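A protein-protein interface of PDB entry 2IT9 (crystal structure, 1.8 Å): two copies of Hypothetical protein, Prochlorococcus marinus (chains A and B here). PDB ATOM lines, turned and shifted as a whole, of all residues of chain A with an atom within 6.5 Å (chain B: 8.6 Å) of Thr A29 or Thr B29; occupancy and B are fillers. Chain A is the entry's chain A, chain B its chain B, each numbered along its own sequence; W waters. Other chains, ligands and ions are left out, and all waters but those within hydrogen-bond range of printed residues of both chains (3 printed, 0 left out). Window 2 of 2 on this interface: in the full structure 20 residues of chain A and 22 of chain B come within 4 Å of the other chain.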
ATOM      1  N   GLY A   9     -24.078 -13.120  23.273  1.00  0.00           N
ATOM      2  CA  GLY A   9     -24.159 -11.906  22.473  1.00  0.00           C
ATOM      3  C   GLY A   9     -25.474 -11.583  21.796  1.00  0.00           C
ATOM      4  O   GLY A   9     -25.574 -10.565  21.128  1.00  0.00           O
ATOM      5  N   GLY A  26     -32.083  -8.464  20.702  1.00  0.00           N
ATOM      6  CA  GLY A  26     -31.001  -8.009  21.539  1.00  0.00           C
ATOM      7  C   GLY A  26     -29.586  -8.404  21.150  1.00  0.00           C
ATOM      8  O   GLY A  26     -29.388  -9.471  20.607  1.00  0.00           O
ATOM      9  N   GLY A  27     -28.632  -7.495  21.415  1.00  0.00           N
ATOM     10  CA  GLY A  27     -27.202  -7.722  21.308  1.00  0.00           C
ATOM     11  C   GLY A  27     -26.608  -7.760  22.723  1.00  0.00           C
ATOM     12  O   GLY A  27     -27.325  -7.881  23.724  1.00  0.00           O
ATOM     13  N   GLU A  28     -25.297  -7.657  22.850  1.00  0.00           N
ATOM     14  CA  GLU A  28     -24.706  -7.713  24.187  1.00  0.00           C
ATOM     15  C   GLU A  28     -25.092  -6.507  25.052  1.00  0.00           C
ATOM     16  O   GLU A  28     -25.356  -6.651  26.247  1.00  0.00           O
ATOM     17  CB  GLU A  28     -23.195  -7.738  24.100  1.00  0.00           C
ATOM     18  CG  GLU A  28     -22.541  -8.042  25.429  1.00  0.00           C
ATOM     19  CD  GLU A  28     -21.046  -8.092  25.359  1.00  0.00           C
ATOM     20  OE1 GLU A  28     -20.464  -7.421  24.482  1.00  0.00           O
ATOM     21  OE2 GLU A  28     -20.451  -8.782  26.222  1.00  0.00           O
ATOM     22  N   THR A  29     -25.105  -5.335  24.433  1.00  0.00           N
ATOM     23  CA  THR A  29     -25.303  -4.076  25.155  1.00  0.00           C
ATOM     24  C   THR A  29     -26.573  -3.317  24.760  1.00  0.00           C
ATOM     25  O   THR A  29     -26.691  -2.118  25.047  1.00  0.00           O
ATOM     26  CB  THR A  29     -24.091  -3.152  24.908  1.00  0.00           C
ATOM     27  OG1 THR A  29     -24.029  -2.746  23.524  1.00  0.00           O
ATOM     28  CG2 THR A  29     -22.781  -3.794  25.342  1.00  0.00           C
ATOM     29  N   TRP A  30     -27.510  -3.976  24.076  1.00  0.00           N
ATOM     30  CA  TRP A  30     -28.712  -3.281  23.641  1.00  0.00           C
ATOM     31  C   TRP A  30     -29.832  -4.265  23.368  1.00  0.00           C
ATOM     32  O   TRP A  30     -29.592  -5.447  23.183  1.00  0.00           O
ATOM     33  CB  TRP A  30     -28.434  -2.511  22.316  1.00  0.00           C
ATOM     34  CG  TRP A  30     -27.908  -3.439  21.168  1.00  0.00           C
ATOM     35  CD1 TRP A  30     -26.616  -3.685  20.853  1.00  0.00           C
ATOM     36  CD2 TRP A  30     -28.702  -4.218  20.237  1.00  0.00           C
ATOM     37  NE1 TRP A  30     -26.531  -4.566  19.794  1.00  0.00           N
ATOM     38  CE2 TRP A  30     -27.798  -4.939  19.417  1.00  0.00           C
ATOM     39  CE3 TRP A  30     -30.076  -4.427  20.070  1.00  0.00           C
ATOM     40  CZ2 TRP A  30     -28.233  -5.834  18.424  1.00  0.00           C
ATOM     41  CZ3 TRP A  30     -30.511  -5.342  19.078  1.00  0.00           C
ATOM     42  CH2 TRP A  30     -29.589  -6.021  18.270  1.00  0.00           C
ATOM     43  N   ALA A  31     -31.054  -3.742  23.387  1.00  0.00           N
ATOM     44  CA  ALA A  31     -32.245  -4.484  22.953  1.00  0.00           C
ATOM     45  C   ALA A  31     -33.242  -3.453  22.478  1.00  0.00           C
ATOM     46  O   ALA A  31     -33.272  -2.344  23.015  1.00  0.00           O
ATOM     47  CB  ALA A  31     -32.813  -5.291  24.061  1.00  0.00           C
ATOM     48  N   GLU A 103     -30.536   2.159  15.784  1.00  0.00           N
ATOM     49  CA  GLU A 103     -29.474   1.527  15.046  1.00  0.00           C
ATOM     50  C   GLU A 103     -28.882   0.502  15.996  1.00  0.00           C
ATOM     51  O   GLU A 103     -28.651   0.776  17.168  1.00  0.00           O
ATOM     52  CB  GLU A 103     -28.414   2.552  14.635  1.00  0.00           C
ATOM     53  CG  GLU A 103     -28.939   3.775  13.938  1.00  0.00           C
ATOM     54  CD  GLU A 103     -27.817   4.754  13.583  1.00  0.00           C
ATOM     55  OE1 GLU A 103     -26.648   4.431  13.900  1.00  0.00           O
ATOM     56  OE2 GLU A 103     -28.106   5.831  13.010  1.00  0.00           O
ATOM     57  N   VAL A 104     -28.663  -0.710  15.507  1.00  0.00           N
ATOM     58  CA  VAL A 104     -28.127  -1.780  16.315  1.00  0.00           C
ATOM     59  C   VAL A 104     -27.120  -2.585  15.501  1.00  0.00           C
ATOM     60  O   VAL A 104     -27.070  -2.468  14.257  1.00  0.00           O
ATOM     61  CB  VAL A 104     -29.233  -2.672  16.899  1.00  0.00           C
ATOM     62  CG1 VAL A 104     -30.196  -1.859  17.772  1.00  0.00           C
ATOM     63  CG2 VAL A 104     -30.018  -3.368  15.801  1.00  0.00           C
ATOM     64  N   TYR A 105     -26.387  -3.451  16.199  1.00  0.00           N
ATOM     65  CA  TYR A 105     -25.267  -4.183  15.561  1.00  0.00           C
ATOM     66  C   TYR A 105     -24.987  -5.517  16.220  1.00  0.00           C
ATOM     67  O   TYR A 105     -25.018  -5.622  17.468  1.00  0.00           O
ATOM     68  CB  TYR A 105     -24.033  -3.305  15.601  1.00  0.00           C
ATOM     69  CG  TYR A 105     -22.722  -3.968  15.242  1.00  0.00           C
ATOM     70  CD1 TYR A 105     -22.269  -3.963  13.917  1.00  0.00           C
ATOM     71  CD2 TYR A 105     -21.924  -4.543  16.212  1.00  0.00           C
ATOM     72  CE1 TYR A 105     -21.026  -4.527  13.575  1.00  0.00           C
ATOM     73  CE2 TYR A 105     -20.678  -5.118  15.876  1.00  0.00           C
ATOM     74  CZ  TYR A 105     -20.260  -5.103  14.550  1.00  0.00           C
ATOM     75  OH  TYR A 105     -19.042  -5.658  14.183  1.00  0.00           O
ATOM     76  N   TRP A 106     -24.765  -6.548  15.389  1.00  0.00           N
ATOM     77  CA  TRP A 106     -24.304  -7.867  15.851  1.00  0.00           C
ATOM     78  C   TRP A 106     -22.959  -8.147  15.189  1.00  0.00           C
ATOM     79  O   TRP A 106     -22.798  -7.896  13.982  1.00  0.00           O
ATOM     80  CB  TRP A 106     -25.243  -9.014  15.496  1.00  0.00           C
ATOM     81  CG  TRP A 106     -26.503  -9.086  16.314  1.00  0.00           C
ATOM     82  CD1 TRP A 106     -26.585  -9.346  17.648  1.00  0.00           C
ATOM     83  CD2 TRP A 106     -27.854  -9.010  15.830  1.00  0.00           C
ATOM     84  NE1 TRP A 106     -27.905  -9.415  18.035  1.00  0.00           N
ATOM     85  CE2 TRP A 106     -28.707  -9.188  16.945  1.00  0.00           C
ATOM     86  CE3 TRP A 106     -28.423  -8.792  14.572  1.00  0.00           C
ATOM     87  CZ2 TRP A 106     -30.101  -9.167  16.827  1.00  0.00           C
ATOM     88  CZ3 TRP A 106     -29.800  -8.761  14.453  1.00  0.00           C
ATOM     89  CH2 TRP A 106     -30.629  -8.965  15.557  1.00  0.00           C
ATOM     90  N   GLY B   9     -17.111   5.536  21.973  1.00  0.00           N
ATOM     91  CA  GLY B   9     -18.162   4.744  22.546  1.00  0.00           C
ATOM     92  C   GLY B   9     -19.441   5.460  22.900  1.00  0.00           C
ATOM     93  O   GLY B   9     -20.284   4.860  23.510  1.00  0.00           O
ATOM     94  N   TRP B  10     -19.625   6.718  22.498  1.00  0.00           N
ATOM     95  CA  TRP B  10     -20.863   7.395  22.832  1.00  0.00           C
ATOM     96  C   TRP B  10     -21.138   8.610  21.973  1.00  0.00           C
ATOM     97  O   TRP B  10     -20.242   9.180  21.355  1.00  0.00           O
ATOM     98  CB  TRP B  10     -20.874   7.840  24.313  1.00  0.00           C
ATOM     99  CG  TRP B  10     -19.864   8.939  24.584  1.00  0.00           C
ATOM    100  CD1 TRP B  10     -18.539   8.774  24.824  1.00  0.00           C
ATOM    101  CD2 TRP B  10     -20.096  10.345  24.572  1.00  0.00           C
ATOM    102  NE1 TRP B  10     -17.922   9.991  24.982  1.00  0.00           N
ATOM    103  CE2 TRP B  10     -18.861  10.974  24.835  1.00  0.00           C
ATOM    104  CE3 TRP B  10     -21.233  11.143  24.367  1.00  0.00           C
ATOM    105  CZ2 TRP B  10     -18.723  12.361  24.898  1.00  0.00           C
ATOM    106  CZ3 TRP B  10     -21.093  12.530  24.440  1.00  0.00           C
ATOM    107  CH2 TRP B  10     -19.847  13.118  24.700  1.00  0.00           C
ATOM    108  N   ARG B  11     -22.425   8.971  21.926  1.00  0.00           N
ATOM    109  CA  ARG B  11     -22.825  10.181  21.229  1.00  0.00           C
ATOM    110  C   ARG B  11     -24.172  10.615  21.701  1.00  0.00           C
ATOM    111  O   ARG B  11     -24.952   9.778  22.160  1.00  0.00           O
ATOM    112  CB  ARG B  11     -22.830  10.007  19.724  1.00  0.00           C
ATOM    113  CG  ARG B  11     -23.757   8.972  19.217  1.00  0.00           C
ATOM    114  CD  ARG B  11     -23.589   8.767  17.708  1.00  0.00           C
ATOM    115  NE  ARG B  11     -24.199   7.513  17.265  1.00  0.00           N
ATOM    116  CZ  ARG B  11     -24.718   7.310  16.059  1.00  0.00           C
ATOM    117  NH1 ARG B  11     -24.772   8.285  15.158  1.00  0.00           N
ATOM    118  NH2 ARG B  11     -25.245   6.144  15.766  1.00  0.00           N
ATOM    119  N   ILE B  25     -29.369   9.168  21.296  1.00  0.00           N
ATOM    120  CA  ILE B  25     -28.328   8.713  22.201  1.00  0.00           C
ATOM    121  C   ILE B  25     -27.711   7.452  21.595  1.00  0.00           C
ATOM    122  O   ILE B  25     -28.416   6.613  21.003  1.00  0.00           O
ATOM    123  CB  ILE B  25     -28.768   8.471  23.689  1.00  0.00           C
ATOM    124  CG1 ILE B  25     -29.914   7.476  23.822  1.00  0.00           C
ATOM    125  CG2 ILE B  25     -29.120   9.774  24.368  1.00  0.00           C
ATOM    126  CD1 ILE B  25     -30.107   7.019  25.177  1.00  0.00           C
ATOM    127  N   GLY B  26     -26.399   7.347  21.695  1.00  0.00           N
ATOM    128  CA  GLY B  26     -25.696   6.183  21.204  1.00  0.00           C
ATOM    129  C   GLY B  26     -24.548   5.670  22.035  1.00  0.00           C
ATOM    130  O   GLY B  26     -23.939   6.420  22.807  1.00  0.00           O
ATOM    131  N   GLY B  27     -24.287   4.367  21.880  1.00  0.00           N
ATOM    132  CA  GLY B  27     -23.170   3.698  22.473  1.00  0.00           C
ATOM    133  C   GLY B  27     -22.323   3.138  21.370  1.00  0.00           C
ATOM    134  O   GLY B  27     -22.455   3.547  20.193  1.00  0.00           O
ATOM    135  N   GLU B  28     -21.447   2.186  21.693  1.00  0.00           N
ATOM    136  CA  GLU B  28     -20.576   1.646  20.664  1.00  0.00           C
ATOM    137  C   GLU B  28     -21.326   0.833  19.629  1.00  0.00           C
ATOM    138  O   GLU B  28     -20.999   0.910  18.465  1.00  0.00           O
ATOM    139  CB  GLU B  28     -19.480   0.757  21.264  1.00  0.00           C
ATOM    140  CG  GLU B  28     -18.450   0.331  20.264  1.00  0.00           C
ATOM    141  CD  GLU B  28     -17.366  -0.515  20.894  1.00  0.00           C
ATOM    142  OE1 GLU B  28     -17.664  -1.173  21.901  1.00  0.00           O
ATOM    143  OE2 GLU B  28     -16.239  -0.552  20.383  1.00  0.00           O
ATOM    144  N   THR B  29     -22.289   0.029  20.052  1.00  0.00           N
ATOM    145  CA  THR B  29     -23.018  -0.838  19.081  1.00  0.00           C
ATOM    146  C   THR B  29     -24.522  -0.573  18.941  1.00  0.00           C
ATOM    147  O   THR B  29     -25.240  -1.423  18.448  1.00  0.00           O
ATOM    148  CB  THR B  29     -22.870  -2.288  19.525  1.00  0.00           C
ATOM    149  OG1 THR B  29     -23.433  -2.397  20.835  1.00  0.00           O
ATOM    150  CG2 THR B  29     -21.394  -2.689  19.517  1.00  0.00           C
ATOM    151  N   TRP B  30     -24.994   0.593  19.374  1.00  0.00           N
ATOM    152  CA  TRP B  30     -26.409   0.905  19.399  1.00  0.00           C
ATOM    153  C   TRP B  30     -26.625   2.419  19.414  1.00  0.00           C
ATOM    154  O   TRP B  30     -25.736   3.195  19.787  1.00  0.00           O
ATOM    155  CB  TRP B  30     -27.094   0.271  20.650  1.00  0.00           C
ATOM    156  CG  TRP B  30     -26.513   0.766  21.985  1.00  0.00           C
ATOM    157  CD1 TRP B  30     -25.498   0.176  22.706  1.00  0.00           C
ATOM    158  CD2 TRP B  30     -26.804   2.012  22.656  1.00  0.00           C
ATOM    159  NE1 TRP B  30     -25.193   0.937  23.805  1.00  0.00           N
ATOM    160  CE2 TRP B  30     -25.981   2.067  23.806  1.00  0.00           C
ATOM    161  CE3 TRP B  30     -27.756   3.020  22.460  1.00  0.00           C
ATOM    162  CZ2 TRP B  30     -26.025   3.125  24.692  1.00  0.00           C
ATOM    163  CZ3 TRP B  30     -27.791   4.100  23.352  1.00  0.00           C
ATOM    164  CH2 TRP B  30     -26.936   4.127  24.457  1.00  0.00           C
ATOM    165  N   ALA B  31     -27.812   2.802  18.989  1.00  0.00           N
ATOM    166  CA  ALA B  31     -28.302   4.147  19.124  1.00  0.00           C
ATOM    167  C   ALA B  31     -29.831   4.098  19.131  1.00  0.00           C
ATOM    168  O   ALA B  31     -30.416   3.281  18.425  1.00  0.00           O
ATOM    169  CB  ALA B  31     -27.808   5.000  17.994  1.00  0.00           C
ATOM    170  N   ILE B  32     -30.479   4.979  19.897  1.00  0.00           N
ATOM    171  CA  ILE B  32     -31.939   5.096  19.876  1.00  0.00           C
ATOM    172  C   ILE B  32     -32.341   6.568  19.884  1.00  0.00           C
ATOM    173  O   ILE B  32     -31.632   7.406  20.434  1.00  0.00           O
ATOM    174  CB  ILE B  32     -32.634   4.347  21.051  1.00  0.00           C
ATOM    175  CG1 ILE B  32     -32.168   4.860  22.439  1.00  0.00           C
ATOM    176  CG2 ILE B  32     -32.416   2.838  20.958  1.00  0.00           C
ATOM    177  CD1 ILE B  32     -32.977   4.325  23.585  1.00  0.00           C
ATOM    178  N   LEU B  88     -23.734   1.651  33.271  1.00  0.00           N
ATOM    179  CA  LEU B  88     -25.098   2.066  33.389  1.00  0.00           C
ATOM    180  C   LEU B  88     -25.937   1.325  32.360  1.00  0.00           C
ATOM    181  O   LEU B  88     -25.611   1.361  31.216  1.00  0.00           O
ATOM    182  CB  LEU B  88     -25.233   3.548  33.073  1.00  0.00           C
ATOM    183  CG  LEU B  88     -26.618   4.197  33.239  1.00  0.00           C
ATOM    184  CD1 LEU B  88     -27.104   4.185  34.680  1.00  0.00           C
ATOM    185  CD2 LEU B  88     -26.550   5.603  32.715  1.00  0.00           C
ATOM    186  N   ARG B  89     -26.999   0.690  32.825  1.00  0.00           N
ATOM    187  CA  ARG B  89     -27.953  -0.006  31.984  1.00  0.00           C
ATOM    188  C   ARG B  89     -29.233   0.791  32.093  1.00  0.00           C
ATOM    189  O   ARG B  89     -29.663   1.120  33.209  1.00  0.00           O
ATOM    190  CB  ARG B  89     -28.133  -1.409  32.503  1.00  0.00           C
ATOM    191  CG  ARG B  89     -29.012  -2.247  31.626  1.00  0.00           C
ATOM    192  CD  ARG B  89     -29.262  -3.614  32.251  1.00  0.00           C
ATOM    193  NE  ARG B  89     -30.252  -4.348  31.475  1.00  0.00           N
ATOM    194  CZ  ARG B  89     -31.036  -5.320  31.944  1.00  0.00           C
ATOM    195  NH1 ARG B  89     -30.991  -5.726  33.214  1.00  0.00           N
ATOM    196  NH2 ARG B  89     -31.903  -5.880  31.127  1.00  0.00           N
ATOM    197  N   LEU B  90     -29.884   1.063  30.963  1.00  0.00           N
ATOM    198  CA  LEU B  90     -31.085   1.880  30.946  1.00  0.00           C
ATOM    199  C   LEU B  90     -32.191   1.085  30.286  1.00  0.00           C
ATOM    200  O   LEU B  90     -31.961   0.508  29.213  1.00  0.00           O
ATOM    201  CB  LEU B  90     -30.826   3.163  30.176  1.00  0.00           C
ATOM    202  CG  LEU B  90     -29.930   4.216  30.848  1.00  0.00           C
ATOM    203  CD1 LEU B  90     -29.501   5.266  29.813  1.00  0.00           C
ATOM    204  CD2 LEU B  90     -30.692   4.818  32.007  1.00  0.00           C
ATOM    205  N   ALA B 102     -36.901  -0.165  24.722  1.00  0.00           N
ATOM    206  CA  ALA B 102     -35.498  -0.425  24.421  1.00  0.00           C
ATOM    207  C   ALA B 102     -34.715  -0.581  25.713  1.00  0.00           C
ATOM    208  O   ALA B 102     -35.191  -0.186  26.772  1.00  0.00           O
ATOM    209  CB  ALA B 102     -34.921   0.717  23.608  1.00  0.00           C
ATOM    210  N   GLU B 103     -33.514  -1.131  25.607  1.00  0.00           N
ATOM    211  CA  GLU B 103     -32.600  -1.306  26.739  1.00  0.00           C
ATOM    212  C   GLU B 103     -31.225  -0.981  26.155  1.00  0.00           C
ATOM    213  O   GLU B 103     -30.891  -1.427  25.049  1.00  0.00           O
ATOM    214  CB  GLU B 103     -32.621  -2.723  27.253  1.00  0.00           C
ATOM    215  CG  GLU B 103     -33.983  -3.204  27.696  1.00  0.00           C
ATOM    216  CD  GLU B 103     -33.951  -4.595  28.249  1.00  0.00           C
ATOM    217  OE1 GLU B 103     -32.839  -5.147  28.358  1.00  0.00           O
ATOM    218  OE2 GLU B 103     -35.018  -5.133  28.602  1.00  0.00           O
ATOM    219  N   VAL B 104     -30.461  -0.144  26.842  1.00  0.00           N
ATOM    220  CA  VAL B 104     -29.179   0.268  26.316  1.00  0.00           C
ATOM    221  C   VAL B 104     -28.189   0.317  27.466  1.00  0.00           C
ATOM    222  O   VAL B 104     -28.587   0.313  28.615  1.00  0.00           O
ATOM    223  CB  VAL B 104     -29.291   1.610  25.574  1.00  0.00           C
ATOM    224  CG1 VAL B 104     -30.353   1.514  24.384  1.00  0.00           C
ATOM    225  CG2 VAL B 104     -29.644   2.736  26.478  1.00  0.00           C
ATOM    226  N   TYR B 105     -26.914   0.402  27.136  1.00  0.00           N
ATOM    227  CA  TYR B 105     -25.872   0.306  28.152  1.00  0.00           C
ATOM    228  C   TYR B 105     -24.615   0.996  27.762  1.00  0.00           C
ATOM    229  O   TYR B 105     -24.180   0.895  26.600  1.00  0.00           O
ATOM    230  CB  TYR B 105     -25.574  -1.160  28.364  1.00  0.00           C
ATOM    231  CG  TYR B 105     -24.338  -1.520  29.155  1.00  0.00           C
ATOM    232  CD1 TYR B 105     -24.420  -1.799  30.523  1.00  0.00           C
ATOM    233  CD2 TYR B 105     -23.100  -1.674  28.532  1.00  0.00           C
ATOM    234  CE1 TYR B 105     -23.295  -2.176  31.246  1.00  0.00           C
ATOM    235  CE2 TYR B 105     -21.969  -2.060  29.266  1.00  0.00           C
ATOM    236  CZ  TYR B 105     -22.089  -2.300  30.608  1.00  0.00           C
ATOM    237  OH  TYR B 105     -21.006  -2.687  31.353  1.00  0.00           O
ATOM    238  N   TRP B 106     -24.021   1.708  28.717  1.00  0.00           N
ATOM    239  CA  TRP B 106     -22.710   2.310  28.524  1.00  0.00           C
ATOM    240  C   TRP B 106     -21.774   1.698  29.580  1.00  0.00           C
ATOM    241  O   TRP B 106     -22.186   1.497  30.735  1.00  0.00           O
ATOM    242  CB  TRP B 106     -22.740   3.828  28.713  1.00  0.00           C
ATOM    243  CG  TRP B 106     -23.318   4.635  27.571  1.00  0.00           C
ATOM    244  CD1 TRP B 106     -22.783   4.794  26.328  1.00  0.00           C
ATOM    245  CD2 TRP B 106     -24.456   5.465  27.630  1.00  0.00           C
ATOM    246  NE1 TRP B 106     -23.561   5.642  25.582  1.00  0.00           N
ATOM    247  CE2 TRP B 106     -24.594   6.080  26.361  1.00  0.00           C
ATOM    248  CE3 TRP B 106     -25.379   5.767  28.632  1.00  0.00           C
ATOM    249  CZ2 TRP B 106     -25.622   6.979  26.067  1.00  0.00           C
ATOM    250  CZ3 TRP B 106     -26.400   6.642  28.340  1.00  0.00           C
ATOM    251  CH2 TRP B 106     -26.522   7.242  27.060  1.00  0.00           C
ATOM    252  N   PRO B 107     -20.535   1.365  29.188  1.00  0.00           N
ATOM    253  CA  PRO B 107     -19.617   0.706  30.101  1.00  0.00           C
ATOM    254  C   PRO B 107     -18.873   1.675  30.995  1.00  0.00           C
ATOM    255  O   PRO B 107     -18.997   2.892  30.851  1.00  0.00           O
ATOM    256  CB  PRO B 107     -18.651   0.024  29.162  1.00  0.00           C
ATOM    257  CG  PRO B 107     -18.544   1.010  28.006  1.00  0.00           C
ATOM    258  CD  PRO B 107     -19.930   1.552  27.861  1.00  0.00           C
HETATM  259  O   HOH W   1     -22.096  -0.881  22.969  1.00  0.00           O
HETATM  260  O   HOH W   2     -26.276   7.636  12.636  1.00  0.00           O
HETATM  261  O   HOH W   3     -23.465  -5.147  21.684  1.00  0.00           O
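Among the printed residues, merely in contact across the chains: Thr A29 with Trp B30 (3.4 Å), Thr A29 with Val B104 (3.7 Å), Trp A30 with Thr B29 (3.4 Å), Trp A30 with Trp B30 (3.5 Å), Trp A30 with Glu B103 (3.2 Å), Ala A31 with Ala B102 (3.3 Å), Glu A103 with Trp B30 (3.2 Å) and Val A104 with Thr B29 (3.6 Å).
Water W2 bridges the side-chain carboxylate (OE2) of Glu A103 (2.6 Å) and the guanidinium group (NH1) of Arg B11 (3.0 Å). Water W1 lies within hydrogen-bond range of the side-chain hydroxyl (OG1) of Thr A29, the side-chain hydroxyl (OG1) of Thr B29 and the backbone NH (N) of Glu B28. Water W3 lies within hydrogen-bond range of the side-chain hydroxyl of Thr B29 (2.9 Å), the side-chain hydroxyl of Thr A29 (3.1 Å) and the backbone NH of Glu A28 (3.3 Å).
Of the 11 printed residues of chain A, 6 touch a printed residue of chain B. Hydrophobic or aromatic side chains of chain A that line the printed part of chain B: Trp A30 and Tyr A105. Hydrophobic or aromatic side chains of chain B within 4 Å of the printed part of chain A: Trp B30, Ala B102 and Tyr B105.
The indole nitrogen (NE1) of Trp A30 lies within hydrogen-bond range of the backbone carbonyl oxygen (O) of Tyr A105, 3.0 Å away. The backbone NH (N) of Gly B26 sits at hydrogen-bond distance from the backbone carbonyl oxygen (O) of Arg B11, 2.9 Å away. The backbone carbonyl oxygen (O) of Tyr B105 sits at hydrogen-bond distance from the indole nitrogen (NE1) of Trp B30, at 3.0 Å. OE1 of Glu B103 is in salt-bridge range of NH2 of Arg B89, at 3.0 Å. O of Val B104 sits at hydrogen-bond distance from N of Leu B90, 2.8 Å away.
Of chain B, only Thr B29, Trp B30, Val B104 and Tyr B105 come within 4 Å of Thr A29. Of the printed residues of chain B, Trp A30 touches Thr B29 (3.4 Å), Trp B30 (3.5 Å) and Glu B103 (3.2 Å). Printed residues of chain B within 4 Å of Ala A31: Ala B102 (3.3 Å) and Glu B103 (2.9 Å). Of the printed residues of chain A, Arg B11 touches Glu A103. Of the printed residues of chain A, Thr B29 touches Thr A29, Trp A30, Val A104 and Tyr A105. Of the printed residues of chain A, Ala B31 touches Glu A103. Of the printed residues of chain A, Ala B102 touches Ala A31. The nearest residue of chain B that does not touch Thr A29 is Glu B103 (4.3 Å). The nearest residue of chain A that does not touch Thr B29 is Glu A103 (4.3 Å).
OG1 of Thr B29 lies within hydrogen-bond range of OG1 of Thr A29. The backbone NH (N) of Tyr B105 lies within hydrogen-bond range of the backbone carbonyl oxygen (O) of Thr A29, 3.3 Å away. O of Glu B103 lies within hydrogen-bond range of N of Ala A31, 2.9 Å away. OE1 of Glu A103 lies within salt-bridge range of NH2 of Arg B11 (2.9 Å). The backbone NH (N) of Ala B31 lies within hydrogen-bond range of the backbone carbonyl oxygen (O) of Glu A103. The backbone NH (N) of Tyr A105 lies within hydrogen-bond range of the backbone carbonyl oxygen (O) of Thr B29 (3.2 Å).
Thr A29 touches its own counterpart, Thr B29. Thr A29 touches Tyr B105, and with the chains exchanged Tyr A105 touches Thr B29. Trp A30 touches its own counterpart, Trp B30. Ala A31 touches Glu B103, and with the chains exchanged Glu A103 touches Ala B31. 11 positions are printed for both chains. Of the 14 pairs that touch across the chains among the printed residues, 12 have their exchanged pair printed and touching as well.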
